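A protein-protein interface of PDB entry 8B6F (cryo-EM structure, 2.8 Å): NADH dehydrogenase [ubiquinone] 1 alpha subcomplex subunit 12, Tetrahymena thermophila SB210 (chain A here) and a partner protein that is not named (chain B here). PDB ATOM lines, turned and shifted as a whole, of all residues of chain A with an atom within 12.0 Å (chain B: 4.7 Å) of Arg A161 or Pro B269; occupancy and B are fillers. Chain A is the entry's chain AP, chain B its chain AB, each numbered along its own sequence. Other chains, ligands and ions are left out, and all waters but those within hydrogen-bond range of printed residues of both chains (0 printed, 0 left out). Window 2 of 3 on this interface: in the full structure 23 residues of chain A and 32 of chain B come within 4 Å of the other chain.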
ATOM      1  N   MET A 150      37.014  29.534  20.365  1.00  0.00           N
ATOM      2  CA  MET A 150      36.523  28.344  19.679  1.00  0.00           C
ATOM      3  C   MET A 150      35.289  27.778  20.366  1.00  0.00           C
ATOM      4  O   MET A 150      34.334  27.366  19.699  1.00  0.00           O
ATOM      5  CB  MET A 150      37.626  27.288  19.607  1.00  0.00           C
ATOM      6  CG  MET A 150      38.759  27.628  18.649  1.00  0.00           C
ATOM      7  SD  MET A 150      38.235  27.705  16.923  1.00  0.00           S
ATOM      8  CE  MET A 150      38.059  29.473  16.689  1.00  0.00           C
ATOM      9  N   ARG A 151      35.290  27.744  21.699  1.00  0.00           N
ATOM     10  CA  ARG A 151      34.139  27.211  22.420  1.00  0.00           C
ATOM     11  C   ARG A 151      32.886  28.021  22.119  1.00  0.00           C
ATOM     12  O   ARG A 151      31.827  27.460  21.811  1.00  0.00           O
ATOM     13  CB  ARG A 151      34.425  27.196  23.922  1.00  0.00           C
ATOM     14  CG  ARG A 151      33.289  26.627  24.752  1.00  0.00           C
ATOM     15  CD  ARG A 151      33.603  26.672  26.238  1.00  0.00           C
ATOM     16  NE  ARG A 151      32.543  26.059  27.028  1.00  0.00           N
ATOM     17  CZ  ARG A 151      32.541  25.980  28.352  1.00  0.00           C
ATOM     18  NH1 ARG A 151      33.530  26.478  29.075  1.00  0.00           N
ATOM     19  NH2 ARG A 151      31.523  25.383  28.965  1.00  0.00           N
ATOM     20  N   PHE A 152      32.984  29.348  22.205  1.00  0.00           N
ATOM     21  CA  PHE A 152      31.824  30.191  21.943  1.00  0.00           C
ATOM     22  C   PHE A 152      31.349  30.042  20.503  1.00  0.00           C
ATOM     23  O   PHE A 152      30.143  29.956  20.246  1.00  0.00           O
ATOM     24  CB  PHE A 152      32.162  31.650  22.251  1.00  0.00           C
ATOM     25  CG  PHE A 152      31.042  32.605  21.962  1.00  0.00           C
ATOM     26  CD1 PHE A 152      30.031  32.806  22.885  1.00  0.00           C
ATOM     27  CD2 PHE A 152      31.006  33.311  20.770  1.00  0.00           C
ATOM     28  CE1 PHE A 152      29.000  33.688  22.624  1.00  0.00           C
ATOM     29  CE2 PHE A 152      29.977  34.194  20.504  1.00  0.00           C
ATOM     30  CZ  PHE A 152      28.975  34.383  21.432  1.00  0.00           C
ATOM     31  N   ILE A 153      32.283  30.010  19.550  1.00  0.00           N
ATOM     32  CA  ILE A 153      31.903  29.899  18.145  1.00  0.00           C
ATOM     33  C   ILE A 153      31.218  28.566  17.882  1.00  0.00           C
ATOM     34  O   ILE A 153      30.197  28.502  17.187  1.00  0.00           O
ATOM     35  CB  ILE A 153      33.138  30.096  17.243  1.00  0.00           C
ATOM     36  CG1 ILE A 153      33.639  31.537  17.350  1.00  0.00           C
ATOM     37  CG2 ILE A 153      32.811  29.755  15.791  1.00  0.00           C
ATOM     38  CD1 ILE A 153      35.000  31.760  16.735  1.00  0.00           C
ATOM     39  N   THR A 154      31.768  27.479  18.425  1.00  0.00           N
ATOM     40  CA  THR A 154      31.149  26.173  18.234  1.00  0.00           C
ATOM     41  C   THR A 154      29.763  26.123  18.864  1.00  0.00           C
ATOM     42  O   THR A 154      28.826  25.572  18.275  1.00  0.00           O
ATOM     43  CB  THR A 154      32.042  25.079  18.821  1.00  0.00           C
ATOM     44  OG1 THR A 154      33.305  25.075  18.144  1.00  0.00           O
ATOM     45  CG2 THR A 154      31.390  23.709  18.675  1.00  0.00           C
ATOM     46  N   ALA A 155      29.609  26.700  20.056  1.00  0.00           N
ATOM     47  CA  ALA A 155      28.300  26.708  20.698  1.00  0.00           C
ATOM     48  C   ALA A 155      27.289  27.492  19.874  1.00  0.00           C
ATOM     49  O   ALA A 155      26.152  27.046  19.688  1.00  0.00           O
ATOM     50  CB  ALA A 155      28.411  27.290  22.107  1.00  0.00           C
ATOM     51  N   GLN A 156      27.685  28.658  19.362  1.00  0.00           N
ATOM     52  CA  GLN A 156      26.771  29.446  18.542  1.00  0.00           C
ATOM     53  C   GLN A 156      26.387  28.694  17.275  1.00  0.00           C
ATOM     54  O   GLN A 156      25.223  28.717  16.859  1.00  0.00           O
ATOM     55  CB  GLN A 156      27.406  30.792  18.197  1.00  0.00           C
ATOM     56  CG  GLN A 156      27.538  31.726  19.385  1.00  0.00           C
ATOM     57  CD  GLN A 156      26.194  32.162  19.929  1.00  0.00           C
ATOM     58  OE1 GLN A 156      25.202  32.206  19.202  1.00  0.00           O
ATOM     59  NE2 GLN A 156      26.151  32.481  21.217  1.00  0.00           N
ATOM     60  N   ARG A 157      27.353  28.024  16.647  1.00  0.00           N
ATOM     61  CA  ARG A 157      27.056  27.247  15.449  1.00  0.00           C
ATOM     62  C   ARG A 157      26.128  26.083  15.769  1.00  0.00           C
ATOM     63  O   ARG A 157      25.227  25.765  14.984  1.00  0.00           O
ATOM     64  CB  ARG A 157      28.355  26.748  14.816  1.00  0.00           C
ATOM     65  CG  ARG A 157      28.162  25.956  13.529  1.00  0.00           C
ATOM     66  CD  ARG A 157      28.219  24.458  13.774  1.00  0.00           C
ATOM     67  NE  ARG A 157      29.521  24.027  14.267  1.00  0.00           N
ATOM     68  CZ  ARG A 157      30.573  23.774  13.501  1.00  0.00           C
ATOM     69  NH1 ARG A 157      30.521  23.908  12.187  1.00  0.00           N
ATOM     70  NH2 ARG A 157      31.708  23.377  14.069  1.00  0.00           N
ATOM     71  N   ASP A 158      26.333  25.432  16.917  1.00  0.00           N
ATOM     72  CA  ASP A 158      25.524  24.268  17.264  1.00  0.00           C
ATOM     73  C   ASP A 158      24.109  24.655  17.673  1.00  0.00           C
ATOM     74  O   ASP A 158      23.191  23.834  17.558  1.00  0.00           O
ATOM     75  CB  ASP A 158      26.196  23.480  18.386  1.00  0.00           C
ATOM     76  CG  ASP A 158      27.548  22.929  17.983  1.00  0.00           C
ATOM     77  OD1 ASP A 158      27.974  23.184  16.837  1.00  0.00           O
ATOM     78  OD2 ASP A 158      28.185  22.241  18.808  1.00  0.00           O
ATOM     79  N   ARG A 159      23.907  25.881  18.165  1.00  0.00           N
ATOM     80  CA  ARG A 159      22.554  26.314  18.503  1.00  0.00           C
ATOM     81  C   ARG A 159      21.609  26.148  17.323  1.00  0.00           C
ATOM     82  O   ARG A 159      20.430  25.827  17.509  1.00  0.00           O
ATOM     83  CB  ARG A 159      22.559  27.774  18.965  1.00  0.00           C
ATOM     84  CG  ARG A 159      23.151  27.989  20.347  1.00  0.00           C
ATOM     85  CD  ARG A 159      22.829  29.371  20.899  1.00  0.00           C
ATOM     86  NE  ARG A 159      21.514  29.417  21.530  1.00  0.00           N
ATOM     87  CZ  ARG A 159      20.395  29.813  20.936  1.00  0.00           C
ATOM     88  NH1 ARG A 159      20.383  30.215  19.676  1.00  0.00           N
ATOM     89  NH2 ARG A 159      19.259  29.807  21.627  1.00  0.00           N
ATOM     90  N   SER A 160      22.106  26.357  16.105  1.00  0.00           N
ATOM     91  CA  SER A 160      21.301  26.220  14.899  1.00  0.00           C
ATOM     92  C   SER A 160      21.572  24.932  14.137  1.00  0.00           C
ATOM     93  O   SER A 160      20.658  24.401  13.498  1.00  0.00           O
ATOM     94  CB  SER A 160      21.552  27.410  13.966  1.00  0.00           C
ATOM     95  OG  SER A 160      20.817  27.280  12.761  1.00  0.00           O
ATOM     96  N   ARG A 161      22.800  24.421  14.188  1.00  0.00           N
ATOM     97  CA  ARG A 161      23.166  23.241  13.406  1.00  0.00           C
ATOM     98  C   ARG A 161      24.413  22.637  14.036  1.00  0.00           C
ATOM     99  O   ARG A 161      25.475  23.266  14.023  1.00  0.00           O
ATOM    100  CB  ARG A 161      23.409  23.619  11.949  1.00  0.00           C
ATOM    101  CG  ARG A 161      24.531  24.640  11.763  1.00  0.00           C
ATOM    102  CD  ARG A 161      24.382  25.425  10.473  1.00  0.00           C
ATOM    103  NE  ARG A 161      23.167  26.231  10.463  1.00  0.00           N
ATOM    104  CZ  ARG A 161      22.824  27.059   9.486  1.00  0.00           C
ATOM    105  NH1 ARG A 161      23.588  27.227   8.420  1.00  0.00           N
ATOM    106  NH2 ARG A 161      21.683  27.735   9.582  1.00  0.00           N
ATOM    107  N   ALA A 162      24.290  21.427  14.580  1.00  0.00           N
ATOM    108  CA  ALA A 162      25.418  20.760  15.212  1.00  0.00           C
ATOM    109  C   ALA A 162      25.990  19.725  14.258  1.00  0.00           C
ATOM    110  O   ALA A 162      25.260  18.805  13.859  1.00  0.00           O
ATOM    111  CB  ALA A 162      24.994  20.098  16.517  1.00  0.00           C
ATOM    112  N   PRO A 163      27.257  19.823  13.855  1.00  0.00           N
ATOM    113  CA  PRO A 163      27.805  18.826  12.929  1.00  0.00           C
ATOM    114  C   PRO A 163      27.765  17.425  13.519  1.00  0.00           C
ATOM    115  O   PRO A 163      27.885  17.233  14.731  1.00  0.00           O
ATOM    116  CB  PRO A 163      29.248  19.297  12.710  1.00  0.00           C
ATOM    117  CG  PRO A 163      29.242  20.737  13.065  1.00  0.00           C
ATOM    118  CD  PRO A 163      28.236  20.881  14.160  1.00  0.00           C
ATOM    119  N   TRP A 164      27.578  16.440  12.644  1.00  0.00           N
ATOM    120  CA  TRP A 164      27.606  15.043  13.055  1.00  0.00           C
ATOM    121  C   TRP A 164      29.043  14.597  13.286  1.00  0.00           C
ATOM    122  O   TRP A 164      29.908  14.793  12.426  1.00  0.00           O
ATOM    123  CB  TRP A 164      26.944  14.170  11.991  1.00  0.00           C
ATOM    124  CG  TRP A 164      27.139  12.700  12.194  1.00  0.00           C
ATOM    125  CD1 TRP A 164      26.690  11.951  13.239  1.00  0.00           C
ATOM    126  CD2 TRP A 164      27.822  11.797  11.315  1.00  0.00           C
ATOM    127  NE1 TRP A 164      27.057  10.636  13.071  1.00  0.00           N
ATOM    128  CE2 TRP A 164      27.753  10.516  11.897  1.00  0.00           C
ATOM    129  CE3 TRP A 164      28.488  11.948  10.094  1.00  0.00           C
ATOM    130  CZ2 TRP A 164      28.325   9.393  11.303  1.00  0.00           C
ATOM    131  CZ3 TRP A 164      29.056  10.830   9.504  1.00  0.00           C
ATOM    132  CH2 TRP A 164      28.970   9.570  10.109  1.00  0.00           C
ATOM    133  N   GLN A 165      29.299  13.998  14.447  1.00  0.00           N
ATOM    134  CA  GLN A 165      30.646  13.556  14.798  1.00  0.00           C
ATOM    135  C   GLN A 165      30.914  12.225  14.111  1.00  0.00           C
ATOM    136  O   GLN A 165      30.426  11.179  14.542  1.00  0.00           O
ATOM    137  CB  GLN A 165      30.790  13.432  16.310  1.00  0.00           C
ATOM    138  CG  GLN A 165      30.506  14.717  17.077  1.00  0.00           C
ATOM    139  CD  GLN A 165      31.485  15.832  16.753  1.00  0.00           C
ATOM    140  OE1 GLN A 165      31.587  16.278  15.611  1.00  0.00           O
ATOM    141  NE2 GLN A 165      32.212  16.290  17.768  1.00  0.00           N
ATOM    142  N   ARG B 267      13.855  33.186  13.300  1.00  0.00           N
ATOM    143  CA  ARG B 267      14.572  34.396  13.687  1.00  0.00           C
ATOM    144  C   ARG B 267      15.996  34.235  13.161  1.00  0.00           C
ATOM    145  O   ARG B 267      16.883  33.752  13.865  1.00  0.00           O
ATOM    146  CB  ARG B 267      14.550  34.603  15.197  1.00  0.00           C
ATOM    147  CG  ARG B 267      15.273  35.861  15.645  1.00  0.00           C
ATOM    148  CD  ARG B 267      15.473  35.890  17.148  1.00  0.00           C
ATOM    149  NE  ARG B 267      16.228  37.066  17.559  1.00  0.00           N
ATOM    150  CZ  ARG B 267      16.640  37.300  18.797  1.00  0.00           C
ATOM    151  NH1 ARG B 267      16.389  36.453  19.782  1.00  0.00           N
ATOM    152  NH2 ARG B 267      17.323  38.411  19.054  1.00  0.00           N
ATOM    153  N   GLY B 268      16.208  34.649  11.916  1.00  0.00           N
ATOM    154  CA  GLY B 268      17.475  34.438  11.261  1.00  0.00           C
ATOM    155  C   GLY B 268      17.650  32.985  10.867  1.00  0.00           C
ATOM    156  O   GLY B 268      16.698  32.322  10.444  1.00  0.00           O
ATOM    157  N   PRO B 269      18.869  32.457  10.993  1.00  0.00           N
ATOM    158  CA  PRO B 269      19.084  31.050  10.621  1.00  0.00           C
ATOM    159  C   PRO B 269      18.232  30.073  11.409  1.00  0.00           C
ATOM    160  O   PRO B 269      17.859  29.022  10.875  1.00  0.00           O
ATOM    161  CB  PRO B 269      20.581  30.840  10.900  1.00  0.00           C
ATOM    162  CG  PRO B 269      21.175  32.197  10.869  1.00  0.00           C
ATOM    163  CD  PRO B 269      20.123  33.117  11.394  1.00  0.00           C
ATOM    164  N   GLU B 270      17.907  30.385  12.661  1.00  0.00           N
ATOM    165  CA  GLU B 270      17.251  29.430  13.541  1.00  0.00           C
ATOM    166  C   GLU B 270      15.763  29.321  13.234  1.00  0.00           C
ATOM    167  O   GLU B 270      15.083  30.326  13.010  1.00  0.00           O
ATOM    168  CB  GLU B 270      17.454  29.839  15.000  1.00  0.00           C
ATOM    169  CG  GLU B 270      18.912  30.042  15.372  1.00  0.00           C
ATOM    170  CD  GLU B 270      19.101  30.393  16.831  1.00  0.00           C
ATOM    171  OE1 GLU B 270      18.142  30.227  17.611  1.00  0.00           O
ATOM    172  OE2 GLU B 270      20.209  30.836  17.198  1.00  0.00           O
ATOM    173  N   ILE B 271      15.260  28.085  13.235  1.00  0.00           N
ATOM    174  CA  ILE B 271      13.850  27.794  13.005  1.00  0.00           C
ATOM    175  C   ILE B 271      13.199  27.472  14.342  1.00  0.00           C
ATOM    176  O   ILE B 271      13.830  26.913  15.247  1.00  0.00           O
ATOM    177  CB  ILE B 271      13.670  26.629  12.006  1.00  0.00           C
ATOM    178  CG1 ILE B 271      14.283  26.987  10.648  1.00  0.00           C
ATOM    179  CG2 ILE B 271      12.197  26.280  11.855  1.00  0.00           C
ATOM    180  CD1 ILE B 271      14.322  25.836   9.665  1.00  0.00           C
ATOM    181  N   LYS B 299      18.512  20.482  13.666  1.00  0.00           N
ATOM    182  CA  LYS B 299      19.453  21.330  14.383  1.00  0.00           C
ATOM    183  C   LYS B 299      20.713  20.597  14.823  1.00  0.00           C
ATOM    184  O   LYS B 299      21.622  21.239  15.360  1.00  0.00           O
ATOM    185  CB  LYS B 299      18.771  21.946  15.608  1.00  0.00           C
ATOM    186  CG  LYS B 299      17.554  22.790  15.278  1.00  0.00           C
ATOM    187  CD  LYS B 299      16.937  23.369  16.538  1.00  0.00           C
ATOM    188  CE  LYS B 299      15.702  24.192  16.219  1.00  0.00           C
ATOM    189  NZ  LYS B 299      15.065  24.731  17.453  1.00  0.00           N
ATOM    190  N   VAL B 604      15.458  28.356   5.044  1.00  0.00           N
ATOM    191  CA  VAL B 604      16.859  28.682   5.282  1.00  0.00           C
ATOM    192  C   VAL B 604      17.713  27.822   4.362  1.00  0.00           C
ATOM    193  O   VAL B 604      17.322  26.718   3.975  1.00  0.00           O
ATOM    194  CB  VAL B 604      17.266  28.474   6.758  1.00  0.00           C
ATOM    195  CG1 VAL B 604      16.534  29.454   7.654  1.00  0.00           C
ATOM    196  CG2 VAL B 604      16.992  27.045   7.194  1.00  0.00           C
ATOM    197  N   PRO B 606      20.819  25.413   3.008  1.00  0.00           N
ATOM    198  CA  PRO B 606      21.364  24.189   3.602  1.00  0.00           C
ATOM    199  C   PRO B 606      22.548  24.498   4.500  1.00  0.00           C
ATOM    200  O   PRO B 606      23.334  25.410   4.212  1.00  0.00           O
ATOM    201  CB  PRO B 606      21.791  23.362   2.379  1.00  0.00           C
ATOM    202  CG  PRO B 606      20.978  23.889   1.261  1.00  0.00           C
ATOM    203  CD  PRO B 606      20.808  25.349   1.537  1.00  0.00           C
ATOM    204  N   PRO B 607      22.710  23.763   5.600  1.00  0.00           N
ATOM    205  CA  PRO B 607      23.789  24.078   6.539  1.00  0.00           C
ATOM    206  C   PRO B 607      25.163  23.797   5.954  1.00  0.00           C
ATOM    207  O   PRO B 607      25.352  22.875   5.157  1.00  0.00           O
ATOM    208  CB  PRO B 607      23.499  23.159   7.729  1.00  0.00           C
ATOM    209  CG  PRO B 607      22.805  22.001   7.131  1.00  0.00           C
ATOM    210  CD  PRO B 607      21.975  22.552   6.002  1.00  0.00           C
ATOM    211  N   GLY B 608      26.131  24.605   6.373  1.00  0.00           N
ATOM    212  CA  GLY B 608      27.510  24.362   5.984  1.00  0.00           C
ATOM    213  C   GLY B 608      27.682  24.365   4.480  1.00  0.00           C
ATOM    214  O   GLY B 608      27.226  25.272   3.777  1.00  0.00           O
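Among the printed residues, merely in contact across the chains: Arg A161 with Lys B299 (3.2 Å), Ser A160 with Lys B299 (3.4 Å), Arg A161 with Pro B269 (3.5 Å), Arg A161 with Pro B607 (3.7 Å), Asp A158 with Lys B299 (3.7 Å), Ser A160 with Pro B269 (3.9 Å) and Ser A160 with Glu B270 (3.98 Å).
NZ of Lys B299 is in hydrogen-bond range of O of Ile B271, at 3.3 Å. The guanidinium group (NE) of Arg A157 lies within salt-bridge range of the side-chain carboxylate (OD1) of Asp A158 (3.1 Å). The side-chain hydroxyl (OG) of Ser A160 sits at hydrogen-bond distance from the guanidinium group (NH2) of Arg A161 (3.3 Å).
No residue of chain A comes within 4 Å of Gly B268. No residue of chain A comes within 4 Å of Val B604. Of the printed residues of chain B, Asp A158 touches Lys B299 (3.7 Å). Printed residues of chain B within 4 Å of Ser A160: Pro B269 (3.9 Å), Glu B270 (3.98 Å) and Lys B299 (3.4 Å). Of the printed residues of chain A, Lys B299 touches Asp A158 (3.7 Å), Ser A160 (3.4 Å), Arg A161 (3.2 Å) and Ala A162 (2.8 Å). Printed residues of chain A within 4 Å of Glu B270: Arg A159 and Ser A160. Of the printed residues of chain B, Ala A162 touches Lys B299. Trp A164 touches none of the printed residues of chain B. The nearest residue of chain A that does not touch Pro B269 is Arg A159 (7.8 Å). The nearest printed residue of chain B that does not touch Asp A158 is Glu B270 (7.3 Å).
Hydrophobic or aromatic side chains of chain B within 4 Å of the printed part of chain A: Pro B269 and Pro B607. Hydrophobic or aromatic side chains of chain A that line the printed part of chain B: Ala A162.
The side-chain carboxylate (OE2) of Glu B270 lies within salt-bridge range of the guanidinium group (NH1) of Arg A159. The backbone carbonyl oxygen of Lys B299 lies within hydrogen-bond range of the backbone NH of Ala A162 (2.8 Å).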
